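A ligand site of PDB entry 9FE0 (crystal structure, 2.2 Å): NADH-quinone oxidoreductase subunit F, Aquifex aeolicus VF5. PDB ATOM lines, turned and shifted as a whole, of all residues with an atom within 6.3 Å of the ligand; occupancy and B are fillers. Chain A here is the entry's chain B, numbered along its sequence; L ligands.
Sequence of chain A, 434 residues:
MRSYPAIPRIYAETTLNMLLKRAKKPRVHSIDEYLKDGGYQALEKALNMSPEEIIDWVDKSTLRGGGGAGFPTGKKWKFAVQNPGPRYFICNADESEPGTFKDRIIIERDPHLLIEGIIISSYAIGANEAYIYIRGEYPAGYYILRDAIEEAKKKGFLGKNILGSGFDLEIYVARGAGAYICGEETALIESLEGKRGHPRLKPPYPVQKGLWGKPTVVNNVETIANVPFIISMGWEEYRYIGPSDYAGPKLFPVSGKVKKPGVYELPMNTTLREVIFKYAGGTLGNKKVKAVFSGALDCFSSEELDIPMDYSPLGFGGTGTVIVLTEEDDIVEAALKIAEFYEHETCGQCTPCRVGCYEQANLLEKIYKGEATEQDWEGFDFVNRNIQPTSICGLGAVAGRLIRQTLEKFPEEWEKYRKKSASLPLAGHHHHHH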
ATOM      1  N   ILE A 181     -10.809  22.036  19.687  1.00  0.00           N
ATOM      2  CA  ILE A 181      -9.605  22.771  20.066  1.00  0.00           C
ATOM      3  C   ILE A 181      -9.795  23.478  21.409  1.00  0.00           C
ATOM      4  O   ILE A 181      -8.833  23.691  22.146  1.00  0.00           O
ATOM      5  CB  ILE A 181      -9.206  23.775  18.955  1.00  0.00           C
ATOM      6  CG1 ILE A 181      -7.786  24.282  19.149  1.00  0.00           C
ATOM      7  CG2 ILE A 181     -10.216  24.921  18.847  1.00  0.00           C
ATOM      8  CD1 ILE A 181      -6.746  23.184  19.287  1.00  0.00           C
ATOM      9  N   GLY A 197     -11.561  30.017  19.891  1.00  0.00           N
ATOM     10  CA  GLY A 197     -10.673  29.076  20.546  1.00  0.00           C
ATOM     11  C   GLY A 197      -9.353  28.981  19.789  1.00  0.00           C
ATOM     12  O   GLY A 197      -9.161  28.047  19.010  1.00  0.00           O
ATOM     13  N   HIS A 198      -8.483  29.973  20.007  1.00  0.00           N
ATOM     14  CA  HIS A 198      -7.161  30.008  19.401  1.00  0.00           C
ATOM     15  C   HIS A 198      -6.106  29.725  20.481  1.00  0.00           C
ATOM     16  O   HIS A 198      -5.912  30.542  21.377  1.00  0.00           O
ATOM     17  CB  HIS A 198      -6.902  31.371  18.753  1.00  0.00           C
ATOM     18  CG  HIS A 198      -7.456  31.530  17.365  1.00  0.00           C
ATOM     19  ND1 HIS A 198      -7.121  32.603  16.551  1.00  0.00           N
ATOM     20  CD2 HIS A 198      -8.327  30.801  16.655  1.00  0.00           C
ATOM     21  CE1 HIS A 198      -7.753  32.499  15.401  1.00  0.00           C
ATOM     22  NE2 HIS A 198      -8.492  31.405  15.431  1.00  0.00           N
ATOM     23  N   PRO A 199      -5.389  28.587  20.432  1.00  0.00           N
ATOM     24  CA  PRO A 199      -4.284  28.348  21.361  1.00  0.00           C
ATOM     25  C   PRO A 199      -3.224  29.447  21.334  1.00  0.00           C
ATOM     26  O   PRO A 199      -2.993  30.085  20.305  1.00  0.00           O
ATOM     27  CB  PRO A 199      -3.724  27.006  20.888  1.00  0.00           C
ATOM     28  CG  PRO A 199      -4.885  26.340  20.192  1.00  0.00           C
ATOM     29  CD  PRO A 199      -5.606  27.469  19.504  1.00  0.00           C
ATOM     30  N   ARG A 200      -2.602  29.660  22.504  1.00  0.00           N
ATOM     31  CA  ARG A 200      -1.500  30.597  22.657  1.00  0.00           C
ATOM     32  C   ARG A 200      -0.206  29.805  22.873  1.00  0.00           C
ATOM     33  O   ARG A 200      -0.228  28.715  23.433  1.00  0.00           O
ATOM     34  CB  ARG A 200      -1.676  31.508  23.871  1.00  0.00           C
ATOM     35  CG  ARG A 200      -3.041  32.112  24.141  1.00  0.00           C
ATOM     36  CD  ARG A 200      -3.073  32.619  25.601  1.00  0.00           C
ATOM     37  NE  ARG A 200      -4.339  33.174  26.069  1.00  0.00           N
ATOM     38  CZ  ARG A 200      -4.588  33.605  27.312  1.00  0.00           C
ATOM     39  NH1 ARG A 200      -3.741  33.379  28.306  1.00  0.00           N
ATOM     40  NH2 ARG A 200      -5.720  34.256  27.564  1.00  0.00           N
ATOM     41  N   GLU A 345     -10.947  19.933  12.839  1.00  0.00           N
ATOM     42  CA  GLU A 345     -10.692  20.595  14.118  1.00  0.00           C
ATOM     43  C   GLU A 345      -9.415  21.447  14.173  1.00  0.00           C
ATOM     44  O   GLU A 345      -9.150  22.080  15.200  1.00  0.00           O
ATOM     45  CB  GLU A 345     -10.643  19.591  15.281  1.00  0.00           C
ATOM     46  CG  GLU A 345     -11.854  18.679  15.376  1.00  0.00           C
ATOM     47  CD  GLU A 345     -13.175  19.386  15.589  1.00  0.00           C
ATOM     48  OE1 GLU A 345     -13.181  20.592  15.963  1.00  0.00           O
ATOM     49  OE2 GLU A 345     -14.214  18.722  15.372  1.00  0.00           O
ATOM     50  N   THR A 346      -8.599  21.505  13.108  1.00  0.00           N
ATOM     51  CA  THR A 346      -7.511  22.487  13.104  1.00  0.00           C
ATOM     52  C   THR A 346      -8.140  23.879  13.168  1.00  0.00           C
ATOM     53  O   THR A 346      -9.126  24.131  12.483  1.00  0.00           O
ATOM     54  CB  THR A 346      -6.553  22.321  11.921  1.00  0.00           C
ATOM     55  OG1 THR A 346      -5.645  23.417  11.991  1.00  0.00           O
ATOM     56  CG2 THR A 346      -7.229  22.350  10.560  1.00  0.00           C
ATOM     57  N   CYS A 347      -7.606  24.748  14.026  1.00  0.00           N
ATOM     58  CA  CYS A 347      -8.080  26.114  14.165  1.00  0.00           C
ATOM     59  C   CYS A 347      -7.511  27.018  13.071  1.00  0.00           C
ATOM     60  O   CYS A 347      -8.049  28.090  12.808  1.00  0.00           O
ATOM     61  CB  CYS A 347      -7.790  26.647  15.577  1.00  0.00           C
ATOM     62  SG  CYS A 347      -6.088  27.249  15.830  1.00  0.00           S
ATOM     63  N   GLY A 348      -6.383  26.612  12.466  1.00  0.00           N
ATOM     64  CA  GLY A 348      -5.884  27.216  11.240  1.00  0.00           C
ATOM     65  C   GLY A 348      -4.876  28.357  11.437  1.00  0.00           C
ATOM     66  O   GLY A 348      -4.467  28.967  10.445  1.00  0.00           O
ATOM     67  N   GLN A 349      -4.447  28.642  12.676  1.00  0.00           N
ATOM     68  CA  GLN A 349      -3.497  29.712  12.941  1.00  0.00           C
ATOM     69  C   GLN A 349      -2.112  29.399  12.370  1.00  0.00           C
ATOM     70  O   GLN A 349      -1.377  30.315  12.022  1.00  0.00           O
ATOM     71  CB  GLN A 349      -3.227  29.918  14.432  1.00  0.00           C
ATOM     72  CG  GLN A 349      -4.417  30.423  15.251  1.00  0.00           C
ATOM     73  CD  GLN A 349      -4.044  30.746  16.685  1.00  0.00           C
ATOM     74  OE1 GLN A 349      -3.827  29.852  17.530  1.00  0.00           O
ATOM     75  NE2 GLN A 349      -3.986  32.036  16.988  1.00  0.00           N
ATOM     76  N   CYS A 350      -1.735  28.114  12.391  1.00  0.00           N
ATOM     77  CA  CYS A 350      -0.420  27.682  11.942  1.00  0.00           C
ATOM     78  C   CYS A 350      -0.540  27.058  10.553  1.00  0.00           C
ATOM     79  O   CYS A 350      -1.371  26.184  10.346  1.00  0.00           O
ATOM     80  CB  CYS A 350       0.205  26.681  12.920  1.00  0.00           C
ATOM     81  SG  CYS A 350      -0.058  27.069  14.673  1.00  0.00           S
ATOM     82  N   THR A 351       0.326  27.488   9.627  1.00  0.00           N
ATOM     83  CA  THR A 351       0.130  27.210   8.208  1.00  0.00           C
ATOM     84  C   THR A 351       0.283  25.705   7.939  1.00  0.00           C
ATOM     85  O   THR A 351      -0.600  25.117   7.329  1.00  0.00           O
ATOM     86  CB  THR A 351       1.034  28.094   7.335  1.00  0.00           C
ATOM     87  OG1 THR A 351       0.460  29.394   7.323  1.00  0.00           O
ATOM     88  CG2 THR A 351       1.143  27.606   5.901  1.00  0.00           C
ATOM     89  N   CYS A 353      -0.139  23.133   9.877  1.00  0.00           N
ATOM     90  CA  CYS A 353      -1.275  22.480  10.512  1.00  0.00           C
ATOM     91  C   CYS A 353      -2.537  22.745   9.695  1.00  0.00           C
ATOM     92  O   CYS A 353      -3.282  21.826   9.406  1.00  0.00           O
ATOM     93  CB  CYS A 353      -1.463  22.940  11.954  1.00  0.00           C
ATOM     94  SG  CYS A 353      -2.875  22.198  12.813  1.00  0.00           S
ATOM     95  N   ARG A 354      -2.745  24.013   9.309  1.00  0.00           N
ATOM     96  CA  ARG A 354      -3.955  24.375   8.586  1.00  0.00           C
ATOM     97  C   ARG A 354      -4.071  23.587   7.280  1.00  0.00           C
ATOM     98  O   ARG A 354      -5.106  22.981   7.011  1.00  0.00           O
ATOM     99  CB  ARG A 354      -3.969  25.882   8.285  1.00  0.00           C
ATOM    100  CG  ARG A 354      -5.208  26.373   7.558  1.00  0.00           C
ATOM    101  CD  ARG A 354      -5.153  27.877   7.316  1.00  0.00           C
ATOM    102  NE  ARG A 354      -4.042  28.301   6.448  1.00  0.00           N
ATOM    103  CZ  ARG A 354      -2.971  28.974   6.862  1.00  0.00           C
ATOM    104  NH1 ARG A 354      -2.750  29.133   8.162  1.00  0.00           N
ATOM    105  NH2 ARG A 354      -2.097  29.433   5.982  1.00  0.00           N
ATOM    106  N   CYS A 357      -3.505  19.287   7.810  1.00  0.00           N
ATOM    107  CA  CYS A 357      -4.663  18.515   8.265  1.00  0.00           C
ATOM    108  C   CYS A 357      -5.670  18.360   7.122  1.00  0.00           C
ATOM    109  O   CYS A 357      -6.275  17.289   6.955  1.00  0.00           O
ATOM    110  CB  CYS A 357      -5.334  19.146   9.496  1.00  0.00           C
ATOM    111  SG  CYS A 357      -4.351  19.004  11.023  1.00  0.00           S
ATOM    112  N   ILE A 387       2.884  18.201   9.150  1.00  0.00           N
ATOM    113  CA  ILE A 387       1.824  18.953   9.799  1.00  0.00           C
ATOM    114  C   ILE A 387       2.401  19.749  10.978  1.00  0.00           C
ATOM    115  O   ILE A 387       1.935  20.847  11.283  1.00  0.00           O
ATOM    116  CB  ILE A 387       0.701  17.992  10.239  1.00  0.00           C
ATOM    117  CG1 ILE A 387       0.179  17.197   9.026  1.00  0.00           C
ATOM    118  CG2 ILE A 387      -0.407  18.743  10.976  1.00  0.00           C
ATOM    119  CD1 ILE A 387      -0.977  16.259   9.311  1.00  0.00           C
ATOM    120  N   THR A 390       6.328  24.475  13.054  1.00  0.00           N
ATOM    121  CA  THR A 390       5.848  25.800  13.457  1.00  0.00           C
ATOM    122  C   THR A 390       4.568  25.718  14.309  1.00  0.00           C
ATOM    123  O   THR A 390       4.091  26.755  14.763  1.00  0.00           O
ATOM    124  CB  THR A 390       5.641  26.740  12.266  1.00  0.00           C
ATOM    125  OG1 THR A 390       4.425  26.429  11.595  1.00  0.00           O
ATOM    126  CG2 THR A 390       6.789  26.701  11.265  1.00  0.00           C
ATOM    127  N   SER A 391       4.010  24.524  14.537  1.00  0.00           N
ATOM    128  CA  SER A 391       2.766  24.389  15.277  1.00  0.00           C
ATOM    129  C   SER A 391       2.944  24.903  16.708  1.00  0.00           C
ATOM    130  O   SER A 391       3.986  24.674  17.308  1.00  0.00           O
ATOM    131  CB  SER A 391       2.291  22.958  15.310  1.00  0.00           C
ATOM    132  OG  SER A 391       3.214  22.151  16.010  1.00  0.00           O
ATOM    133  N   ILE A 392       1.918  25.565  17.247  1.00  0.00           N
ATOM    134  CA  ILE A 392       2.018  26.127  18.590  1.00  0.00           C
ATOM    135  C   ILE A 392       1.254  25.299  19.617  1.00  0.00           C
ATOM    136  O   ILE A 392       1.280  25.663  20.784  1.00  0.00           O
ATOM    137  CB  ILE A 392       1.621  27.619  18.628  1.00  0.00           C
ATOM    138  CG1 ILE A 392       0.148  27.867  18.311  1.00  0.00           C
ATOM    139  CG2 ILE A 392       2.537  28.463  17.738  1.00  0.00           C
ATOM    140  CD1 ILE A 392      -0.173  29.324  18.014  1.00  0.00           C
ATOM    141  N   CYS A 393       0.577  24.207  19.226  1.00  0.00           N
ATOM    142  CA  CYS A 393      -0.155  23.375  20.178  1.00  0.00           C
ATOM    143  C   CYS A 393      -0.113  21.928  19.721  1.00  0.00           C
ATOM    144  O   CYS A 393       0.359  21.626  18.629  1.00  0.00           O
ATOM    145  CB  CYS A 393      -1.593  23.871  20.412  1.00  0.00           C
ATOM    146  SG  CYS A 393      -2.865  23.141  19.346  1.00  0.00           S
ATOM    147  N   GLY A 394      -0.626  21.039  20.576  1.00  0.00           N
ATOM    148  CA  GLY A 394      -0.431  19.603  20.431  1.00  0.00           C
ATOM    149  C   GLY A 394      -1.255  18.981  19.289  1.00  0.00           C
ATOM    150  O   GLY A 394      -0.942  17.866  18.884  1.00  0.00           O
ATOM    151  N   LEU A 395      -2.280  19.666  18.783  1.00  0.00           N
ATOM    152  CA  LEU A 395      -3.070  19.108  17.683  1.00  0.00           C
ATOM    153  C   LEU A 395      -2.168  18.975  16.464  1.00  0.00           C
ATOM    154  O   LEU A 395      -2.134  17.922  15.814  1.00  0.00           O
ATOM    155  CB  LEU A 395      -4.303  19.977  17.391  1.00  0.00           C
ATOM    156  CG  LEU A 395      -5.326  19.413  16.395  1.00  0.00           C
ATOM    157  CD1 LEU A 395      -6.686  20.084  16.618  1.00  0.00           C
ATOM    158  CD2 LEU A 395      -4.904  19.593  14.949  1.00  0.00           C
ATOM    159  N   GLY A 396      -1.399  20.029  16.175  1.00  0.00           N
ATOM    160  CA  GLY A 396      -0.507  20.045  15.025  1.00  0.00           C
ATOM    161  C   GLY A 396       0.615  19.032  15.216  1.00  0.00           C
ATOM    162  O   GLY A 396       1.044  18.384  14.256  1.00  0.00           O
ATOM    163  N   ALA A 397       1.068  18.873  16.464  1.00  0.00           N
ATOM    164  CA  ALA A 397       2.199  17.990  16.747  1.00  0.00           C
ATOM    165  C   ALA A 397       1.840  16.503  16.580  1.00  0.00           C
ATOM    166  O   ALA A 397       2.732  15.703  16.360  1.00  0.00           O
ATOM    167  CB  ALA A 397       2.728  18.288  18.144  1.00  0.00           C
HETATM  168 FE1  LIG L   1      -4.429  25.743  15.734  1.00  0.00          FE
HETATM  169 FE2  LIG L   1      -3.133  23.607  14.575  1.00  0.00          FE
HETATM  170 FE3  LIG L   1      -2.860  24.105  17.255  1.00  0.00          FE
HETATM  171 FE4  LIG L   1      -1.732  25.783  15.415  1.00  0.00          FE
HETATM  172  S1  LIG L   1      -1.210  23.568  15.782  1.00  0.00           S
HETATM  173  S2  LIG L   1      -2.870  26.384  17.286  1.00  0.00           S
HETATM  174  S3  LIG L   1      -3.263  25.732  13.750  1.00  0.00           S
HETATM  175  S4  LIG L   1      -4.821  23.550  16.153  1.00  0.00           S
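N of Ile 392 sits close to SG of Cys 350 (3.6 Å).
The side-chain sulfur (SG) of Cys 353 lies close to the side-chain hydroxyl (OG1) of Thr 346, at 3.1 Å.
The backbone carbonyl oxygen of Cys 353 sits close to the side-chain sulfur of Cys 357, at 3.4 Å.
N of Cys 353 is in hydrogen-bond range of O of Ile 387 (3.4 Å).
N of Leu 395 sits close to SG of Cys 393.
ND1 of His 198 lies within hydrogen-bond range of NE2 of Gln 349.
The backbone NH of Gly 348 sits at hydrogen-bond distance from the side-chain hydroxyl of Thr 346, 3.3 Å away.
The backbone carbonyl oxygen (O) of Gly 348 lies within hydrogen-bond range of the guanidinium group (NH1) of Arg 354.
CD1 of Ile 181 touches S4 of the ligand, 3.7 Å away.
Pro 199 touches the ligand.
CB of Ser 391 touches S1 of the ligand (3.6 Å).
CG1 of Ile 392 touches S2 of the ligand (3.5 Å).
CB of Leu 395 touches S4 of the ligand (3.8 Å).
Hydrophobic or aromatic side chains that line the ligand: Ile 181, Pro 199, Ile 392 and Leu 395.
13 residues have an atom within 4 Å of the ligand: Ile 181, Pro 199, Thr 346, Cys 347, Gly 348, Gln 349, Cys 350, Cys 353, Ser 391, Ile 392, Cys 393, Leu 395 and Gly 396.
N of Cys 350 lies close to S3 of the ligand, at 3.1 Å.
FE4 of the ligand is bound by SG of Cys 350, at 2.2 Å.
The backbone NH (N) of Cys 347 lies close to a sulfur (S4) of the ligand, 3.7 Å away.
SG of Cys 347 is bound to FE1 of the ligand, 2.2 Å away.
The side-chain sulfur of Cys 353 is bound to an iron atom (FE2) of the ligand (2.3 Å).
An iron atom (FE3) of the ligand is bound by the side-chain sulfur (SG) of Cys 393 (2.3 Å).
N of Gln 349 lies close to S3 of the ligand (3.3 Å).
OE1 of Gln 349 lies close to S2 of the ligand (3.6 Å).
N of Gly 348 sits close to S3 of the ligand (3.5 Å).
The backbone NH (N) of Gly 396 lies close to a sulfur (S1) of the ligand (3.6 Å).
A sulfur (S3) of the ligand sits close to the side-chain hydroxyl of Thr 346, 3.8 Å away.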
